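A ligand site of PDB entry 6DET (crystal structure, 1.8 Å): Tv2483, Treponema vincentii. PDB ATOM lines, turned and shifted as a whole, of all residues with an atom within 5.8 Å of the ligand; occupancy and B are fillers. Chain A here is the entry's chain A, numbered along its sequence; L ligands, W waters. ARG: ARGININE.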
ATOM      1  N   SER A  43      29.706  15.803   3.494  1.00  0.00           N
ATOM      2  CA  SER A  43      28.601  16.740   3.442  1.00  0.00           C
ATOM      3  C   SER A  43      27.663  16.388   4.593  1.00  0.00           C
ATOM      4  O   SER A  43      27.157  15.270   4.683  1.00  0.00           O
ATOM      5  CB  SER A  43      27.877  16.644   2.105  1.00  0.00           C
ATOM      6  OG  SER A  43      28.678  17.073   0.988  1.00  0.00           O
ATOM      7  N   PHE A  45      24.641  17.106   5.411  1.00  0.00           N
ATOM      8  CA  PHE A  45      23.208  17.190   5.173  1.00  0.00           C
ATOM      9  C   PHE A  45      22.692  15.986   4.390  1.00  0.00           C
ATOM     10  O   PHE A  45      21.560  16.025   3.898  1.00  0.00           O
ATOM     11  CB  PHE A  45      22.868  18.482   4.409  1.00  0.00           C
ATOM     12  CG  PHE A  45      23.711  18.703   3.164  1.00  0.00           C
ATOM     13  CD1 PHE A  45      24.821  19.532   3.186  1.00  0.00           C
ATOM     14  CD2 PHE A  45      23.410  18.033   1.980  1.00  0.00           C
ATOM     15  CE1 PHE A  45      25.593  19.724   2.035  1.00  0.00           C
ATOM     16  CE2 PHE A  45      24.201  18.213   0.829  1.00  0.00           C
ATOM     17  CZ  PHE A  45      25.281  19.053   0.859  1.00  0.00           C
ATOM     18  N   VAL A  46      23.473  14.918   4.239  1.00  0.00           N
ATOM     19  CA  VAL A  46      23.011  13.809   3.395  1.00  0.00           C
ATOM     20  C   VAL A  46      22.140  12.875   4.246  1.00  0.00           C
ATOM     21  O   VAL A  46      22.665  12.269   5.178  1.00  0.00           O
ATOM     22  CB  VAL A  46      24.185  13.023   2.785  1.00  0.00           C
ATOM     23  CG1 VAL A  46      23.696  11.873   1.947  1.00  0.00           C
ATOM     24  CG2 VAL A  46      25.062  13.933   1.940  1.00  0.00           C
ATOM     25  N   TRP A  84      31.124  20.246  -1.033  1.00  0.00           N
ATOM     26  CA  TRP A  84      31.338  19.077  -1.870  1.00  0.00           C
ATOM     27  C   TRP A  84      32.192  19.403  -3.086  1.00  0.00           C
ATOM     28  O   TRP A  84      32.985  18.570  -3.534  1.00  0.00           O
ATOM     29  CB  TRP A  84      29.993  18.486  -2.301  1.00  0.00           C
ATOM     30  CG  TRP A  84      30.060  17.064  -2.842  1.00  0.00           C
ATOM     31  CD1 TRP A  84      29.720  16.652  -4.117  1.00  0.00           C
ATOM     32  CD2 TRP A  84      30.447  15.887  -2.134  1.00  0.00           C
ATOM     33  NE1 TRP A  84      29.889  15.293  -4.233  1.00  0.00           N
ATOM     34  CE2 TRP A  84      30.326  14.801  -3.039  1.00  0.00           C
ATOM     35  CE3 TRP A  84      30.879  15.626  -0.830  1.00  0.00           C
ATOM     36  CZ2 TRP A  84      30.639  13.487  -2.684  1.00  0.00           C
ATOM     37  CZ3 TRP A  84      31.180  14.311  -0.467  1.00  0.00           C
ATOM     38  CH2 TRP A  84      31.060  13.265  -1.404  1.00  0.00           C
ATOM     39  N   LYS A  87      35.996  18.971  -2.751  1.00  0.00           N
ATOM     40  CA  LYS A  87      36.449  17.760  -2.100  1.00  0.00           C
ATOM     41  C   LYS A  87      37.802  17.300  -2.635  1.00  0.00           C
ATOM     42  O   LYS A  87      38.642  16.834  -1.878  1.00  0.00           O
ATOM     43  CB  LYS A  87      35.376  16.644  -2.229  1.00  0.00           C
ATOM     44  CG  LYS A  87      34.977  16.233  -3.641  1.00  0.00           C
ATOM     45  CD  LYS A  87      33.803  15.257  -3.597  1.00  0.00           C
ATOM     46  CE  LYS A  87      33.292  14.992  -5.007  1.00  0.00           C
ATOM     47  NZ  LYS A  87      32.678  16.248  -5.573  1.00  0.00           N
ATOM     48  N   ALA A 100      33.603  10.642   2.383  1.00  0.00           N
ATOM     49  CA  ALA A 100      32.458   9.753   2.517  1.00  0.00           C
ATOM     50  C   ALA A 100      31.224  10.565   2.092  1.00  0.00           C
ATOM     51  O   ALA A 100      31.310  11.352   1.151  1.00  0.00           O
ATOM     52  CB  ALA A 100      32.386   9.196   3.950  1.00  0.00           C
ATOM     53  N   SER A 101      30.062  10.361   2.741  1.00  0.00           N
ATOM     54  CA  SER A 101      28.807  11.025   2.370  1.00  0.00           C
ATOM     55  C   SER A 101      28.237  10.524   1.047  1.00  0.00           C
ATOM     56  O   SER A 101      27.636  11.299   0.290  1.00  0.00           O
ATOM     57  CB  SER A 101      28.979  12.562   2.316  1.00  0.00           C
ATOM     58  OG  SER A 101      29.222  12.968   3.612  1.00  0.00           O
ATOM     59  N   GLY A 102      28.385   9.235   0.755  1.00  0.00           N
ATOM     60  CA  GLY A 102      27.773   8.671  -0.434  1.00  0.00           C
ATOM     61  C   GLY A 102      28.539   8.969  -1.707  1.00  0.00           C
ATOM     62  O   GLY A 102      27.967   9.373  -2.719  1.00  0.00           O
ATOM     63  N   PHE A 103      29.865   8.780  -1.654  1.00  0.00           N
ATOM     64  CA  PHE A 103      30.739   9.052  -2.796  1.00  0.00           C
ATOM     65  C   PHE A 103      30.608   7.944  -3.845  1.00  0.00           C
ATOM     66  O   PHE A 103      30.959   6.786  -3.580  1.00  0.00           O
ATOM     67  CB  PHE A 103      32.178   9.192  -2.270  1.00  0.00           C
ATOM     68  CG  PHE A 103      33.175   9.653  -3.308  1.00  0.00           C
ATOM     69  CD1 PHE A 103      33.633  10.970  -3.307  1.00  0.00           C
ATOM     70  CD2 PHE A 103      33.703   8.770  -4.242  1.00  0.00           C
ATOM     71  CE1 PHE A 103      34.547  11.385  -4.257  1.00  0.00           C
ATOM     72  CE2 PHE A 103      34.618   9.194  -5.190  1.00  0.00           C
ATOM     73  CZ  PHE A 103      35.044  10.504  -5.186  1.00  0.00           C
ATOM     74  N   SER A 104      30.165   8.305  -5.053  1.00  0.00           N
ATOM     75  CA  SER A 104      29.982   7.350  -6.148  1.00  0.00           C
ATOM     76  C   SER A 104      31.261   7.032  -6.914  1.00  0.00           C
ATOM     77  O   SER A 104      32.053   7.913  -7.269  1.00  0.00           O
ATOM     78  CB  SER A 104      28.945   7.905  -7.122  1.00  0.00           C
ATOM     79  OG  SER A 104      27.712   8.078  -6.456  1.00  0.00           O
ATOM     80  N   ARG A 109      36.456   9.300 -12.040  1.00  0.00           N
ATOM     81  CA  ARG A 109      37.024   9.453 -10.699  1.00  0.00           C
ATOM     82  C   ARG A 109      38.128   8.440 -10.404  1.00  0.00           C
ATOM     83  O   ARG A 109      38.998   8.705  -9.552  1.00  0.00           O
ATOM     84  CB  ARG A 109      35.925   9.337  -9.669  1.00  0.00           C
ATOM     85  CG  ARG A 109      35.061  10.557  -9.623  1.00  0.00           C
ATOM     86  CD  ARG A 109      33.867  10.383  -8.690  1.00  0.00           C
ATOM     87  NE  ARG A 109      33.123  11.644  -8.535  1.00  0.00           N
ATOM     88  CZ  ARG A 109      32.092  11.827  -7.711  1.00  0.00           C
ATOM     89  NH1 ARG A 109      31.658  10.817  -6.969  1.00  0.00           N
ATOM     90  NH2 ARG A 109      31.515  13.037  -7.620  1.00  0.00           N
ATOM     91  N   ASN A 122      24.009   1.901  -5.483  1.00  0.00           N
ATOM     92  CA  ASN A 122      23.152   3.067  -5.585  1.00  0.00           C
ATOM     93  C   ASN A 122      22.660   3.192  -7.019  1.00  0.00           C
ATOM     94  O   ASN A 122      23.180   2.554  -7.935  1.00  0.00           O
ATOM     95  CB  ASN A 122      23.887   4.330  -5.142  1.00  0.00           C
ATOM     96  CG  ASN A 122      23.024   5.558  -5.283  1.00  0.00           C
ATOM     97  OD1 ASN A 122      21.979   5.673  -4.625  1.00  0.00           O
ATOM     98  ND2 ASN A 122      23.455   6.486  -6.140  1.00  0.00           N
ATOM     99  N   LYS A 124      20.979   6.566  -9.478  1.00  0.00           N
ATOM    100  CA  LYS A 124      20.430   7.909  -9.621  1.00  0.00           C
ATOM    101  C   LYS A 124      19.031   7.769 -10.201  1.00  0.00           C
ATOM    102  O   LYS A 124      18.823   7.055 -11.178  1.00  0.00           O
ATOM    103  CB  LYS A 124      21.307   8.735 -10.540  1.00  0.00           C
ATOM    104  CG  LYS A 124      22.529   9.304  -9.751  1.00  0.00           C
ATOM    105  CD  LYS A 124      23.481  10.076 -10.615  1.00  0.00           C
ATOM    106  CE  LYS A 124      24.635  10.642  -9.789  1.00  0.00           C
ATOM    107  NZ  LYS A 124      25.068   9.756  -8.673  1.00  0.00           N
ATOM    108  N   GLU A 148      22.497  18.194  -7.745  1.00  0.00           N
ATOM    109  CA  GLU A 148      23.509  18.675  -6.821  1.00  0.00           C
ATOM    110  C   GLU A 148      24.833  18.890  -7.571  1.00  0.00           C
ATOM    111  O   GLU A 148      25.272  18.051  -8.364  1.00  0.00           O
ATOM    112  CB  GLU A 148      23.644  17.700  -5.651  1.00  0.00           C
ATOM    113  CG  GLU A 148      24.494  18.214  -4.521  1.00  0.00           C
ATOM    114  CD  GLU A 148      24.616  17.235  -3.333  1.00  0.00           C
ATOM    115  OE1 GLU A 148      24.325  16.017  -3.455  1.00  0.00           O
ATOM    116  OE2 GLU A 148      25.069  17.702  -2.263  1.00  0.00           O
ATOM    117  N   ASP A 150      28.652  19.090  -8.692  1.00  0.00           N
ATOM    118  CA  ASP A 150      29.837  18.244  -8.548  1.00  0.00           C
ATOM    119  C   ASP A 150      29.524  16.838  -8.081  1.00  0.00           C
ATOM    120  O   ASP A 150      30.305  16.226  -7.340  1.00  0.00           O
ATOM    121  CB  ASP A 150      30.859  18.885  -7.603  1.00  0.00           C
ATOM    122  CG  ASP A 150      31.445  20.164  -8.163  1.00  0.00           C
ATOM    123  OD1 ASP A 150      32.496  20.073  -8.834  1.00  0.00           O
ATOM    124  OD2 ASP A 150      30.848  21.236  -7.942  1.00  0.00           O
ATOM    125  N   THR A 151      28.384  16.297  -8.541  1.00  0.00           N
ATOM    126  CA  THR A 151      28.007  14.921  -8.278  1.00  0.00           C
ATOM    127  C   THR A 151      27.953  14.084  -9.549  1.00  0.00           C
ATOM    128  O   THR A 151      27.442  12.947  -9.506  1.00  0.00           O
ATOM    129  CB  THR A 151      26.650  14.837  -7.576  1.00  0.00           C
ATOM    130  OG1 THR A 151      25.646  15.383  -8.452  1.00  0.00           O
ATOM    131  CG2 THR A 151      26.659  15.569  -6.246  1.00  0.00           C
ATOM    132  N   ALA A 152      28.422  14.612 -10.677  1.00  0.00           N
ATOM    133  CA  ALA A 152      28.268  13.961 -11.985  1.00  0.00           C
ATOM    134  C   ALA A 152      26.809  13.651 -12.294  1.00  0.00           C
ATOM    135  O   ALA A 152      26.516  12.724 -13.068  1.00  0.00           O
ATOM    136  CB  ALA A 152      29.091  12.678 -12.086  1.00  0.00           C
ATOM    137  N   ILE A 175      20.986  19.281  -1.077  1.00  0.00           N
ATOM    138  CA  ILE A 175      19.865  18.432  -1.485  1.00  0.00           C
ATOM    139  C   ILE A 175      18.550  19.145  -1.205  1.00  0.00           C
ATOM    140  O   ILE A 175      17.589  19.045  -1.981  1.00  0.00           O
ATOM    141  CB  ILE A 175      19.946  17.082  -0.755  1.00  0.00           C
ATOM    142  CG1 ILE A 175      21.216  16.310  -1.185  1.00  0.00           C
ATOM    143  CG2 ILE A 175      18.689  16.246  -1.008  1.00  0.00           C
ATOM    144  CD1 ILE A 175      21.546  15.131  -0.258  1.00  0.00           C
ATOM    145  N   ASP A 193      20.102  10.549  -5.330  1.00  0.00           N
ATOM    146  CA  ASP A 193      20.560   9.167  -5.162  1.00  0.00           C
ATOM    147  C   ASP A 193      19.493   8.386  -4.418  1.00  0.00           C
ATOM    148  O   ASP A 193      18.963   8.861  -3.398  1.00  0.00           O
ATOM    149  CB  ASP A 193      21.891   9.055  -4.396  1.00  0.00           C
ATOM    150  CG  ASP A 193      23.089   9.589  -5.165  1.00  0.00           C
ATOM    151  OD1 ASP A 193      22.997   9.912  -6.363  1.00  0.00           O
ATOM    152  OD2 ASP A 193      24.193   9.652  -4.537  1.00  0.00           O
ATOM    153  N   TYR A 196      20.142   7.767  -0.292  1.00  0.00           N
ATOM    154  CA  TYR A 196      19.807   8.751   0.737  1.00  0.00           C
ATOM    155  C   TYR A 196      18.355   9.177   0.665  1.00  0.00           C
ATOM    156  O   TYR A 196      17.915   9.916   1.559  1.00  0.00           O
ATOM    157  CB  TYR A 196      20.760   9.976   0.700  1.00  0.00           C
ATOM    158  CG  TYR A 196      20.706  10.902  -0.508  1.00  0.00           C
ATOM    159  CD1 TYR A 196      21.821  11.067  -1.344  1.00  0.00           C
ATOM    160  CD2 TYR A 196      19.581  11.677  -0.762  1.00  0.00           C
ATOM    161  CE1 TYR A 196      21.786  11.924  -2.419  1.00  0.00           C
ATOM    162  CE2 TYR A 196      19.526  12.536  -1.840  1.00  0.00           C
ATOM    163  CZ  TYR A 196      20.615  12.671  -2.668  1.00  0.00           C
ATOM    164  OH  TYR A 196      20.558  13.544  -3.722  1.00  0.00           O
ATOM    165  N   GLU A 217      25.161   2.245  -9.838  1.00  0.00           N
ATOM    166  CA  GLU A 217      26.423   2.733  -9.303  1.00  0.00           C
ATOM    167  C   GLU A 217      26.798   1.926  -8.074  1.00  0.00           C
ATOM    168  O   GLU A 217      25.992   1.195  -7.496  1.00  0.00           O
ATOM    169  CB  GLU A 217      26.368   4.216  -8.839  1.00  0.00           C
ATOM    170  CG  GLU A 217      25.783   5.184  -9.776  1.00  0.00           C
ATOM    171  CD  GLU A 217      25.617   6.604  -9.192  1.00  0.00           C
ATOM    172  OE1 GLU A 217      25.277   7.493 -10.005  1.00  0.00           O
ATOM    173  OE2 GLU A 217      25.725   6.844  -7.965  1.00  0.00           O
ATOM    174  N   TYR A 219      28.838   2.961  -4.272  1.00  0.00           N
ATOM    175  CA  TYR A 219      29.401   3.937  -3.358  1.00  0.00           C
ATOM    176  C   TYR A 219      30.730   3.382  -2.839  1.00  0.00           C
ATOM    177  O   TYR A 219      30.874   2.177  -2.670  1.00  0.00           O
ATOM    178  CB  TYR A 219      28.489   4.174  -2.160  1.00  0.00           C
ATOM    179  CG  TYR A 219      27.286   5.108  -2.358  1.00  0.00           C
ATOM    180  CD1 TYR A 219      27.168   5.911  -3.474  1.00  0.00           C
ATOM    181  CD2 TYR A 219      26.346   5.203  -1.359  1.00  0.00           C
ATOM    182  CE1 TYR A 219      26.073   6.834  -3.591  1.00  0.00           C
ATOM    183  CE2 TYR A 219      25.260   6.078  -1.454  1.00  0.00           C
ATOM    184  CZ  TYR A 219      25.142   6.880  -2.570  1.00  0.00           C
ATOM    185  OH  TYR A 219      24.093   7.787  -2.608  1.00  0.00           O
HETATM  186  N   ARG L   1      26.898  10.323  -4.946  1.00  0.00           N
HETATM  187  CA  ARG L   1      27.194  11.776  -4.964  1.00  0.00           C
HETATM  188  C   ARG L   1      28.623  11.994  -5.419  1.00  0.00           C
HETATM  189  O   ARG L   1      29.433  11.046  -5.335  1.00  0.00           O
HETATM  190  CB  ARG L   1      26.994  12.399  -3.578  1.00  0.00           C
HETATM  191  CG  ARG L   1      25.542  12.404  -3.093  1.00  0.00           C
HETATM  192  CD  ARG L   1      25.375  12.944  -1.679  1.00  0.00           C
HETATM  193  NE  ARG L   1      25.736  14.352  -1.632  1.00  0.00           N
HETATM  194  CZ  ARG L   1      26.838  14.835  -1.057  1.00  0.00           C
HETATM  195  NH1 ARG L   1      27.060  16.143  -1.127  1.00  0.00           N
HETATM  196  NH2 ARG L   1      27.704  14.030  -0.443  1.00  0.00           N
HETATM  197  OXT ARG L   1      28.980  13.107  -5.857  1.00  0.00           O
HETATM  198  O   HOH W   1      24.120  12.431  -6.473  1.00  0.00           O
HETATM  199  O   HOH W   2      27.531  10.844  -7.997  1.00  0.00           O
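A nitrogen (N) of the ligand lies within hydrogen-bond range of the backbone carbonyl oxygen of Gly 102 (2.6 Å).
O of the ligand lies within salt-bridge range of NH1 of Arg 109 (2.8 Å).
NH1 of the ligand lies within salt-bridge range of OE2 of Glu 148 (2.8 Å).
The side-chain carboxylate (OD2) of Asp 193 lies within salt-bridge range of a nitrogen (N) of the ligand, 2.8 Å away.
A nitrogen (NH1) of the ligand lies within hydrogen-bond range of the side-chain hydroxyl (OG) of Ser 43, at 2.8 Å.
O of the ligand lies within hydrogen-bond range of N of Ser 104.
The side-chain hydroxyl (OG) of Ser 104 is in hydrogen-bond range of a nitrogen (N) of the ligand.
O of Ser 101 sits at hydrogen-bond distance from NH2 of the ligand (2.8 Å).
The indole nitrogen of Trp 84 is in hydrogen-bond range of an oxygen (OXT) of the ligand (2.9 Å).
O of Ser 104 lies within hydrogen-bond range of NH1 of Arg 109.
NH2 of Arg 109 sits at hydrogen-bond distance from O of Asp 150 (3.4 Å).
The backbone NH of Asp 193 lies within hydrogen-bond range of the side-chain hydroxyl of Tyr 196, 3.4 Å away.
The side-chain carboxylate (OD1) of Asp 193 is in salt-bridge range of the side-chain amino group (NZ) of Lys 124 (3.1 Å).
The side-chain carboxylate (OD1) of Asp 193 lies close to the side-chain amide nitrogen (ND2) of Asn 122, 3.5 Å away.
The backbone NH (N) of Ser 43 lies within hydrogen-bond range of the side-chain hydroxyl (OG) of Ser 101 (2.9 Å).
The backbone carbonyl oxygen (O) of Trp 84 sits close to the side-chain amino group (NZ) of Lys 87 (3.1 Å).
The side-chain amino group (NZ) of Lys 87 lies within hydrogen-bond range of the backbone carbonyl oxygen (O) of Asp 150, at 3.0 Å.
Phe 45 touches the ligand (CZ to NH1, 3.9 Å).
Val 46 touches the ligand (CG2 to NH2, 3.6 Å).
CA of Phe 103 touches O of the ligand (3.5 Å).
Asp 150 touches the ligand (O to OXT, 3.7 Å).
Thr 151 touches the ligand (CA to OXT, 3.2 Å).
CE1 of Tyr 196 touches CD of the ligand, 3.8 Å away.
Tyr 219 touches the ligand.
Water W2 lies within hydrogen-bond range of O of Thr 151, NZ of Lys 124, N of the ligand and OG of Ser 104.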
